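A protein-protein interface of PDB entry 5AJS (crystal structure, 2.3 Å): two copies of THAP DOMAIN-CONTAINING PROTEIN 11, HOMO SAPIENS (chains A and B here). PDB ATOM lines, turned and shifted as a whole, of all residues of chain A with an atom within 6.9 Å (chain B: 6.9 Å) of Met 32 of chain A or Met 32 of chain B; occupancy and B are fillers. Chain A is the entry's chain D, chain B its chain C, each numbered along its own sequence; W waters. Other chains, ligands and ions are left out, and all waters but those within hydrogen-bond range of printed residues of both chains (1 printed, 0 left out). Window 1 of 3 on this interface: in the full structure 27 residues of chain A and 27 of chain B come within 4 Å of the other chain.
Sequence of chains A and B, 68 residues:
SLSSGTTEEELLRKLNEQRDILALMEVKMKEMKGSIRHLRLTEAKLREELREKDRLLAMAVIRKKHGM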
ATOM      1  N   MET A  25      17.986   0.605  30.503  1.00  0.00           N
ATOM      2  CA  MET A  25      18.816   1.302  29.526  1.00  0.00           C
ATOM      3  C   MET A  25      18.891   0.645  28.155  1.00  0.00           C
ATOM      4  O   MET A  25      19.060   1.329  27.125  1.00  0.00           O
ATOM      5  CB  MET A  25      20.230   1.447  30.081  1.00  0.00           C
ATOM      6  CG  MET A  25      20.366   2.570  31.088  1.00  0.00           C
ATOM      7  SD  MET A  25      22.106   2.760  31.511  1.00  0.00           S
ATOM      8  CE  MET A  25      22.177   4.512  31.898  1.00  0.00           C
ATOM      9  N   VAL A  27      16.341  -0.816  26.827  1.00  0.00           N
ATOM     10  CA  VAL A  27      15.067  -0.458  26.217  1.00  0.00           C
ATOM     11  C   VAL A  27      15.181   0.912  25.526  1.00  0.00           C
ATOM     12  O   VAL A  27      14.957   1.051  24.322  1.00  0.00           O
ATOM     13  CB  VAL A  27      13.952  -0.440  27.296  1.00  0.00           C
ATOM     14  CG1 VAL A  27      12.715   0.303  26.814  1.00  0.00           C
ATOM     15  CG2 VAL A  27      13.594  -1.859  27.697  1.00  0.00           C
ATOM     16  N   LYS A  28      15.529   1.910  26.323  1.00  0.00           N
ATOM     17  CA  LYS A  28      15.720   3.279  25.874  1.00  0.00           C
ATOM     18  C   LYS A  28      16.591   3.281  24.611  1.00  0.00           C
ATOM     19  O   LYS A  28      16.189   3.797  23.571  1.00  0.00           O
ATOM     20  CB  LYS A  28      16.375   4.093  27.007  1.00  0.00           C
ATOM     21  CG  LYS A  28      16.410   5.589  26.820  1.00  0.00           C
ATOM     22  CD  LYS A  28      15.008   6.198  26.772  1.00  0.00           C
ATOM     23  CE  LYS A  28      15.047   7.727  26.716  1.00  0.00           C
ATOM     24  NZ  LYS A  28      13.957   8.348  27.538  1.00  0.00           N
ATOM     25  N   MET A  29      17.759   2.661  24.689  1.00  0.00           N
ATOM     26  CA  MET A  29      18.647   2.587  23.538  1.00  0.00           C
ATOM     27  C   MET A  29      18.019   1.922  22.320  1.00  0.00           C
ATOM     28  O   MET A  29      18.366   2.271  21.188  1.00  0.00           O
ATOM     29  CB  MET A  29      19.921   1.829  23.883  1.00  0.00           C
ATOM     30  CG  MET A  29      20.854   2.618  24.764  1.00  0.00           C
ATOM     31  SD  MET A  29      22.313   1.662  25.220  1.00  0.00           S
ATOM     32  CE  MET A  29      22.922   1.227  23.582  1.00  0.00           C
ATOM     33  N   LYS A  30      17.140   0.937  22.531  1.00  0.00           N
ATOM     34  CA  LYS A  30      16.433   0.330  21.397  1.00  0.00           C
ATOM     35  C   LYS A  30      15.487   1.363  20.828  1.00  0.00           C
ATOM     36  O   LYS A  30      15.425   1.485  19.636  1.00  0.00           O
ATOM     37  CB  LYS A  30      15.688  -0.966  21.736  1.00  0.00           C
ATOM     38  N   GLU A  31      14.791   2.144  21.652  1.00  0.00           N
ATOM     39  CA  GLU A  31      13.929   3.192  21.090  1.00  0.00           C
ATOM     40  C   GLU A  31      14.767   4.241  20.342  1.00  0.00           C
ATOM     41  O   GLU A  31      14.505   4.576  19.184  1.00  0.00           O
ATOM     42  CB  GLU A  31      13.169   3.940  22.170  1.00  0.00           C
ATOM     43  CG  GLU A  31      12.215   3.103  22.999  1.00  0.00           C
ATOM     44  CD  GLU A  31      11.896   3.790  24.323  1.00  0.00           C
ATOM     45  OE1 GLU A  31      12.071   5.040  24.409  1.00  0.00           O
ATOM     46  OE2 GLU A  31      11.489   3.080  25.268  1.00  0.00           O
ATOM     47  N   MET A  32      15.772   4.751  21.038  1.00  0.00           N
ATOM     48  CA  MET A  32      16.638   5.799  20.511  1.00  0.00           C
ATOM     49  C   MET A  32      17.217   5.481  19.126  1.00  0.00           C
ATOM     50  O   MET A  32      17.302   6.370  18.312  1.00  0.00           O
ATOM     51  CB  MET A  32      17.755   6.080  21.508  1.00  0.00           C
ATOM     52  CG  MET A  32      17.284   6.862  22.716  1.00  0.00           C
ATOM     53  SD  MET A  32      18.616   7.090  23.926  1.00  0.00           S
ATOM     54  CE  MET A  32      19.363   8.649  23.431  1.00  0.00           C
ATOM     55  N   LYS A  33      17.597   4.224  18.875  1.00  0.00           N
ATOM     56  CA  LYS A  33      18.140   3.799  17.564  1.00  0.00           C
ATOM     57  C   LYS A  33      17.023   3.583  16.557  1.00  0.00           C
ATOM     58  O   LYS A  33      17.222   3.780  15.372  1.00  0.00           O
ATOM     59  CB  LYS A  33      19.024   2.547  17.657  1.00  0.00           C
ATOM     60  N   GLY A  34      15.837   3.216  17.018  1.00  0.00           N
ATOM     61  CA  GLY A  34      14.662   3.401  16.187  1.00  0.00           C
ATOM     62  C   GLY A  34      14.691   4.842  15.664  1.00  0.00           C
ATOM     63  O   GLY A  34      14.978   5.077  14.489  1.00  0.00           O
ATOM     64  N   SER A  35      14.456   5.788  16.581  1.00  0.00           N
ATOM     65  CA  SER A  35      14.313   7.194  16.267  1.00  0.00           C
ATOM     66  C   SER A  35      15.318   7.624  15.223  1.00  0.00           C
ATOM     67  O   SER A  35      14.952   8.167  14.199  1.00  0.00           O
ATOM     68  CB  SER A  35      14.471   8.051  17.522  1.00  0.00           C
ATOM     69  OG  SER A  35      13.200   8.447  18.042  1.00  0.00           O
ATOM     70  N   ILE A  36      16.584   7.340  15.468  1.00  0.00           N
ATOM     71  CA  ILE A  36      17.625   7.699  14.519  1.00  0.00           C
ATOM     72  C   ILE A  36      17.441   7.139  13.118  1.00  0.00           C
ATOM     73  O   ILE A  36      17.649   7.861  12.143  1.00  0.00           O
ATOM     74  CB  ILE A  36      18.979   7.322  15.077  1.00  0.00           C
ATOM     75  CG1 ILE A  36      19.317   8.283  16.214  1.00  0.00           C
ATOM     76  CG2 ILE A  36      20.046   7.369  14.013  1.00  0.00           C
ATOM     77  CD1 ILE A  36      20.591   7.943  16.969  1.00  0.00           C
ATOM     78  N   ARG A  37      17.035   5.879  12.990  1.00  0.00           N
ATOM     79  CA  ARG A  37      16.779   5.346  11.651  1.00  0.00           C
ATOM     80  C   ARG A  37      15.592   6.052  10.968  1.00  0.00           C
ATOM     81  O   ARG A  37      15.639   6.313   9.783  1.00  0.00           O
ATOM     82  CB  ARG A  37      16.523   3.851  11.692  1.00  0.00           C
ATOM     83  N   LEU A  39      14.658   9.089  11.548  1.00  0.00           N
ATOM     84  CA  LEU A  39      15.021  10.480  11.358  1.00  0.00           C
ATOM     85  C   LEU A  39      15.989  10.587  10.201  1.00  0.00           C
ATOM     86  O   LEU A  39      15.901  11.538   9.416  1.00  0.00           O
ATOM     87  CB  LEU A  39      15.627  11.085  12.630  1.00  0.00           C
ATOM     88  CG  LEU A  39      14.628  11.501  13.727  1.00  0.00           C
ATOM     89  CD1 LEU A  39      15.361  11.842  15.028  1.00  0.00           C
ATOM     90  CD2 LEU A  39      13.789  12.704  13.322  1.00  0.00           C
ATOM     91  N   MET B  25      27.421   2.248  28.124  1.00  0.00           N
ATOM     92  CA  MET B  25      26.070   2.409  27.597  1.00  0.00           C
ATOM     93  C   MET B  25      25.752   3.835  27.779  1.00  0.00           C
ATOM     94  O   MET B  25      25.171   4.454  26.897  1.00  0.00           O
ATOM     95  CB  MET B  25      25.029   1.558  28.357  1.00  0.00           C
ATOM     96  CG  MET B  25      25.116   0.065  28.041  1.00  0.00           C
ATOM     97  SD  MET B  25      23.808  -0.934  28.797  1.00  0.00           S
ATOM     98  CE  MET B  25      22.439  -0.554  27.695  1.00  0.00           C
ATOM     99  N   VAL B  27      27.700   6.322  27.608  1.00  0.00           N
ATOM    100  CA  VAL B  27      28.426   7.019  26.558  1.00  0.00           C
ATOM    101  C   VAL B  27      27.708   6.984  25.199  1.00  0.00           C
ATOM    102  O   VAL B  27      27.698   7.960  24.458  1.00  0.00           O
ATOM    103  CB  VAL B  27      29.828   6.363  26.402  1.00  0.00           C
ATOM    104  CG1 VAL B  27      30.383   6.519  24.998  1.00  0.00           C
ATOM    105  CG2 VAL B  27      30.787   6.939  27.434  1.00  0.00           C
ATOM    106  N   LYS B  28      27.193   5.816  24.850  1.00  0.00           N
ATOM    107  CA  LYS B  28      26.542   5.608  23.598  1.00  0.00           C
ATOM    108  C   LYS B  28      25.233   6.407  23.672  1.00  0.00           C
ATOM    109  O   LYS B  28      24.978   7.258  22.843  1.00  0.00           O
ATOM    110  CB  LYS B  28      26.299   4.118  23.387  1.00  0.00           C
ATOM    111  CG  LYS B  28      25.747   3.746  22.027  1.00  0.00           C
ATOM    112  CD  LYS B  28      26.809   3.909  20.946  1.00  0.00           C
ATOM    113  CE  LYS B  28      26.325   3.493  19.558  1.00  0.00           C
ATOM    114  NZ  LYS B  28      26.041   2.037  19.452  1.00  0.00           N
ATOM    115  N   MET B  29      24.456   6.212  24.721  1.00  0.00           N
ATOM    116  CA  MET B  29      23.238   6.975  24.864  1.00  0.00           C
ATOM    117  C   MET B  29      23.531   8.481  24.690  1.00  0.00           C
ATOM    118  O   MET B  29      22.802   9.178  23.975  1.00  0.00           O
ATOM    119  CB  MET B  29      22.521   6.647  26.198  1.00  0.00           C
ATOM    120  CG  MET B  29      21.884   5.248  26.227  1.00  0.00           C
ATOM    121  SD  MET B  29      21.184   4.707  27.819  1.00  0.00           S
ATOM    122  CE  MET B  29      19.793   5.847  28.011  1.00  0.00           C
ATOM    123  N   LYS B  30      24.621   8.954  25.295  1.00  0.00           N
ATOM    124  CA  LYS B  30      25.079  10.354  25.154  1.00  0.00           C
ATOM    125  C   LYS B  30      25.251  10.775  23.701  1.00  0.00           C
ATOM    126  O   LYS B  30      24.786  11.824  23.281  1.00  0.00           O
ATOM    127  CB  LYS B  30      26.433  10.534  25.866  1.00  0.00           C
ATOM    128  N   GLU B  31      25.955   9.957  22.940  1.00  0.00           N
ATOM    129  CA  GLU B  31      26.148  10.230  21.511  1.00  0.00           C
ATOM    130  C   GLU B  31      24.848  10.092  20.691  1.00  0.00           C
ATOM    131  O   GLU B  31      24.725  10.719  19.630  1.00  0.00           O
ATOM    132  CB  GLU B  31      27.217   9.304  20.924  1.00  0.00           C
ATOM    133  CG  GLU B  31      28.601   9.503  21.530  1.00  0.00           C
ATOM    134  CD  GLU B  31      29.519   8.313  21.300  1.00  0.00           C
ATOM    135  OE1 GLU B  31      29.451   7.715  20.205  1.00  0.00           O
ATOM    136  OE2 GLU B  31      30.306   7.980  22.214  1.00  0.00           O
ATOM    137  N   MET B  32      23.907   9.273  21.178  1.00  0.00           N
ATOM    138  CA  MET B  32      22.637   9.039  20.500  1.00  0.00           C
ATOM    139  C   MET B  32      21.649  10.202  20.707  1.00  0.00           C
ATOM    140  O   MET B  32      20.914  10.557  19.798  1.00  0.00           O
ATOM    141  CB  MET B  32      21.987   7.722  20.987  1.00  0.00           C
ATOM    142  CG  MET B  32      22.417   6.422  20.285  1.00  0.00           C
ATOM    143  SD  MET B  32      21.612   4.997  21.081  1.00  0.00           S
ATOM    144  CE  MET B  32      21.140   4.014  19.656  1.00  0.00           C
ATOM    145  N   LYS B  33      21.594  10.756  21.912  1.00  0.00           N
ATOM    146  CA  LYS B  33      20.655  11.862  22.193  1.00  0.00           C
ATOM    147  C   LYS B  33      21.135  13.171  21.536  1.00  0.00           C
ATOM    148  O   LYS B  33      20.356  14.061  21.237  1.00  0.00           O
ATOM    149  CB  LYS B  33      20.488  12.065  23.693  1.00  0.00           C
ATOM    150  N   GLY B  34      22.439  13.276  21.326  1.00  0.00           N
ATOM    151  CA  GLY B  34      22.975  14.329  20.514  1.00  0.00           C
ATOM    152  C   GLY B  34      22.511  14.170  19.082  1.00  0.00           C
ATOM    153  O   GLY B  34      22.062  15.152  18.472  1.00  0.00           O
ATOM    154  N   SER B  35      22.648  12.947  18.546  1.00  0.00           N
ATOM    155  CA  SER B  35      22.224  12.649  17.178  1.00  0.00           C
ATOM    156  C   SER B  35      20.757  12.967  16.950  1.00  0.00           C
ATOM    157  O   SER B  35      20.373  13.339  15.850  1.00  0.00           O
ATOM    158  CB  SER B  35      22.453  11.173  16.811  1.00  0.00           C
ATOM    159  OG  SER B  35      23.387  11.017  15.746  1.00  0.00           O
ATOM    160  N   ILE B  36      19.932  12.780  17.971  1.00  0.00           N
ATOM    161  CA  ILE B  36      18.517  13.008  17.812  1.00  0.00           C
ATOM    162  C   ILE B  36      18.238  14.502  17.794  1.00  0.00           C
ATOM    163  O   ILE B  36      17.600  14.986  16.863  1.00  0.00           O
ATOM    164  CB  ILE B  36      17.679  12.227  18.864  1.00  0.00           C
ATOM    165  CG1 ILE B  36      17.656  10.734  18.505  1.00  0.00           C
ATOM    166  CG2 ILE B  36      16.220  12.686  18.913  1.00  0.00           C
ATOM    167  CD1 ILE B  36      17.339   9.843  19.691  1.00  0.00           C
ATOM    168  N   ARG B  37      18.739  15.240  18.784  1.00  0.00           N
ATOM    169  CA  ARG B  37      18.490  16.692  18.830  1.00  0.00           C
ATOM    170  C   ARG B  37      18.980  17.374  17.534  1.00  0.00           C
ATOM    171  O   ARG B  37      18.298  18.211  16.977  1.00  0.00           O
ATOM    172  CB  ARG B  37      19.136  17.342  20.055  1.00  0.00           C
ATOM    173  N   LEU B  39      19.138  15.821  14.705  1.00  0.00           N
ATOM    174  CA  LEU B  39      18.289  15.373  13.594  1.00  0.00           C
ATOM    175  C   LEU B  39      16.954  16.101  13.595  1.00  0.00           C
ATOM    176  O   LEU B  39      16.417  16.431  12.541  1.00  0.00           O
ATOM    177  CB  LEU B  39      18.127  13.841  13.584  1.00  0.00           C
ATOM    178  CG  LEU B  39      19.414  13.186  12.986  1.00  0.00           C
ATOM    179  CD1 LEU B  39      19.574  11.666  13.217  1.00  0.00           C
ATOM    180  CD2 LEU B  39      19.529  13.515  11.528  1.00  0.00           C
HETATM  181  O   HOH W   1      16.080  14.927  10.119  1.00  0.00           O
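Among the printed residues, merely in contact across the chains: Met 29 of chain A with Met 29 of chain B (3.2 Å), Lys 33 of chain A with Met 32 of chain B (3.3 Å), Met 29 of chain A with Met 25 of chain B (3.3 Å), Met 32 of chain A with Lys 33 of chain B (3.4 Å), Met 32 of chain A with Met 29 of chain B (3.5 Å), Lys 28 of chain A with Met 29 of chain B (3.6 Å), Met 29 of chain A with Met 32 of chain B (3.6 Å), Met 32 of chain A with Met 32 of chain B (3.7 Å), Leu 39 of chain A with Leu 39 of chain B (3.7 Å), Ile 36 of chain A with Ser 35 of chain B (3.7 Å), Met 32 of chain A with Ile 36 of chain B (3.7 Å), Ile 36 of chain A with Ile 36 of chain B (3.7 Å), Met 25 of chain A with Met 25 of chain B (3.8 Å), Ile 36 of chain A with Met 32 of chain B (3.9 Å) and Met 25 of chain A with Met 29 of chain B (3.99 Å).
Of the printed residues of chain B, Met 32 of chain A touches Met 29, Met 32, Lys 33 and Ile 36.
Printed residues of chain B within 4 Å of Met 29 of chain A: Met 25, Met 29 and Met 32.
Of the printed residues of chain A, Leu 39 of chain B touches Leu 39 (3.7 Å).
The nearest residue of chain A that does not touch Met 32 of chain B is Lys 30 of chain A (5.8 Å).
Hydrophobic or aromatic side chains of chain A that line the printed part of chain B: Met 25, Met 29, Met 32, Ile 36 and Leu 39.
Of the 13 printed residues of chain B, 7 touch a printed residue of chain A.
Hydrophobic or aromatic side chains of chain B within 4 Å of the printed part of chain A: Met 25, Met 29, Met 32, Ile 36 and Leu 39.
Met 25 of chain B touches its own counterpart, Met 25 of chain A.
Lys 28 of chain A touches Met 29 of chain B, but with the chains exchanged Met 29 of chain A does not touch Lys 28 of chain B (4.1 Å).
Met 32 of chain A touches Ile 36 of chain B, and with the chains exchanged Ile 36 of chain A touches Met 32 of chain B.
Leu 39 of chain A touches its own counterpart, Leu 39 of chain B.
13 positions are printed for both chains.
Water W1 lies within hydrogen-bond range of the backbone carbonyl oxygen (O) of Leu 39 of chain B (2.9 Å) and the backbone carbonyl oxygen (O) of Leu 39 of chain A (3.5 Å).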
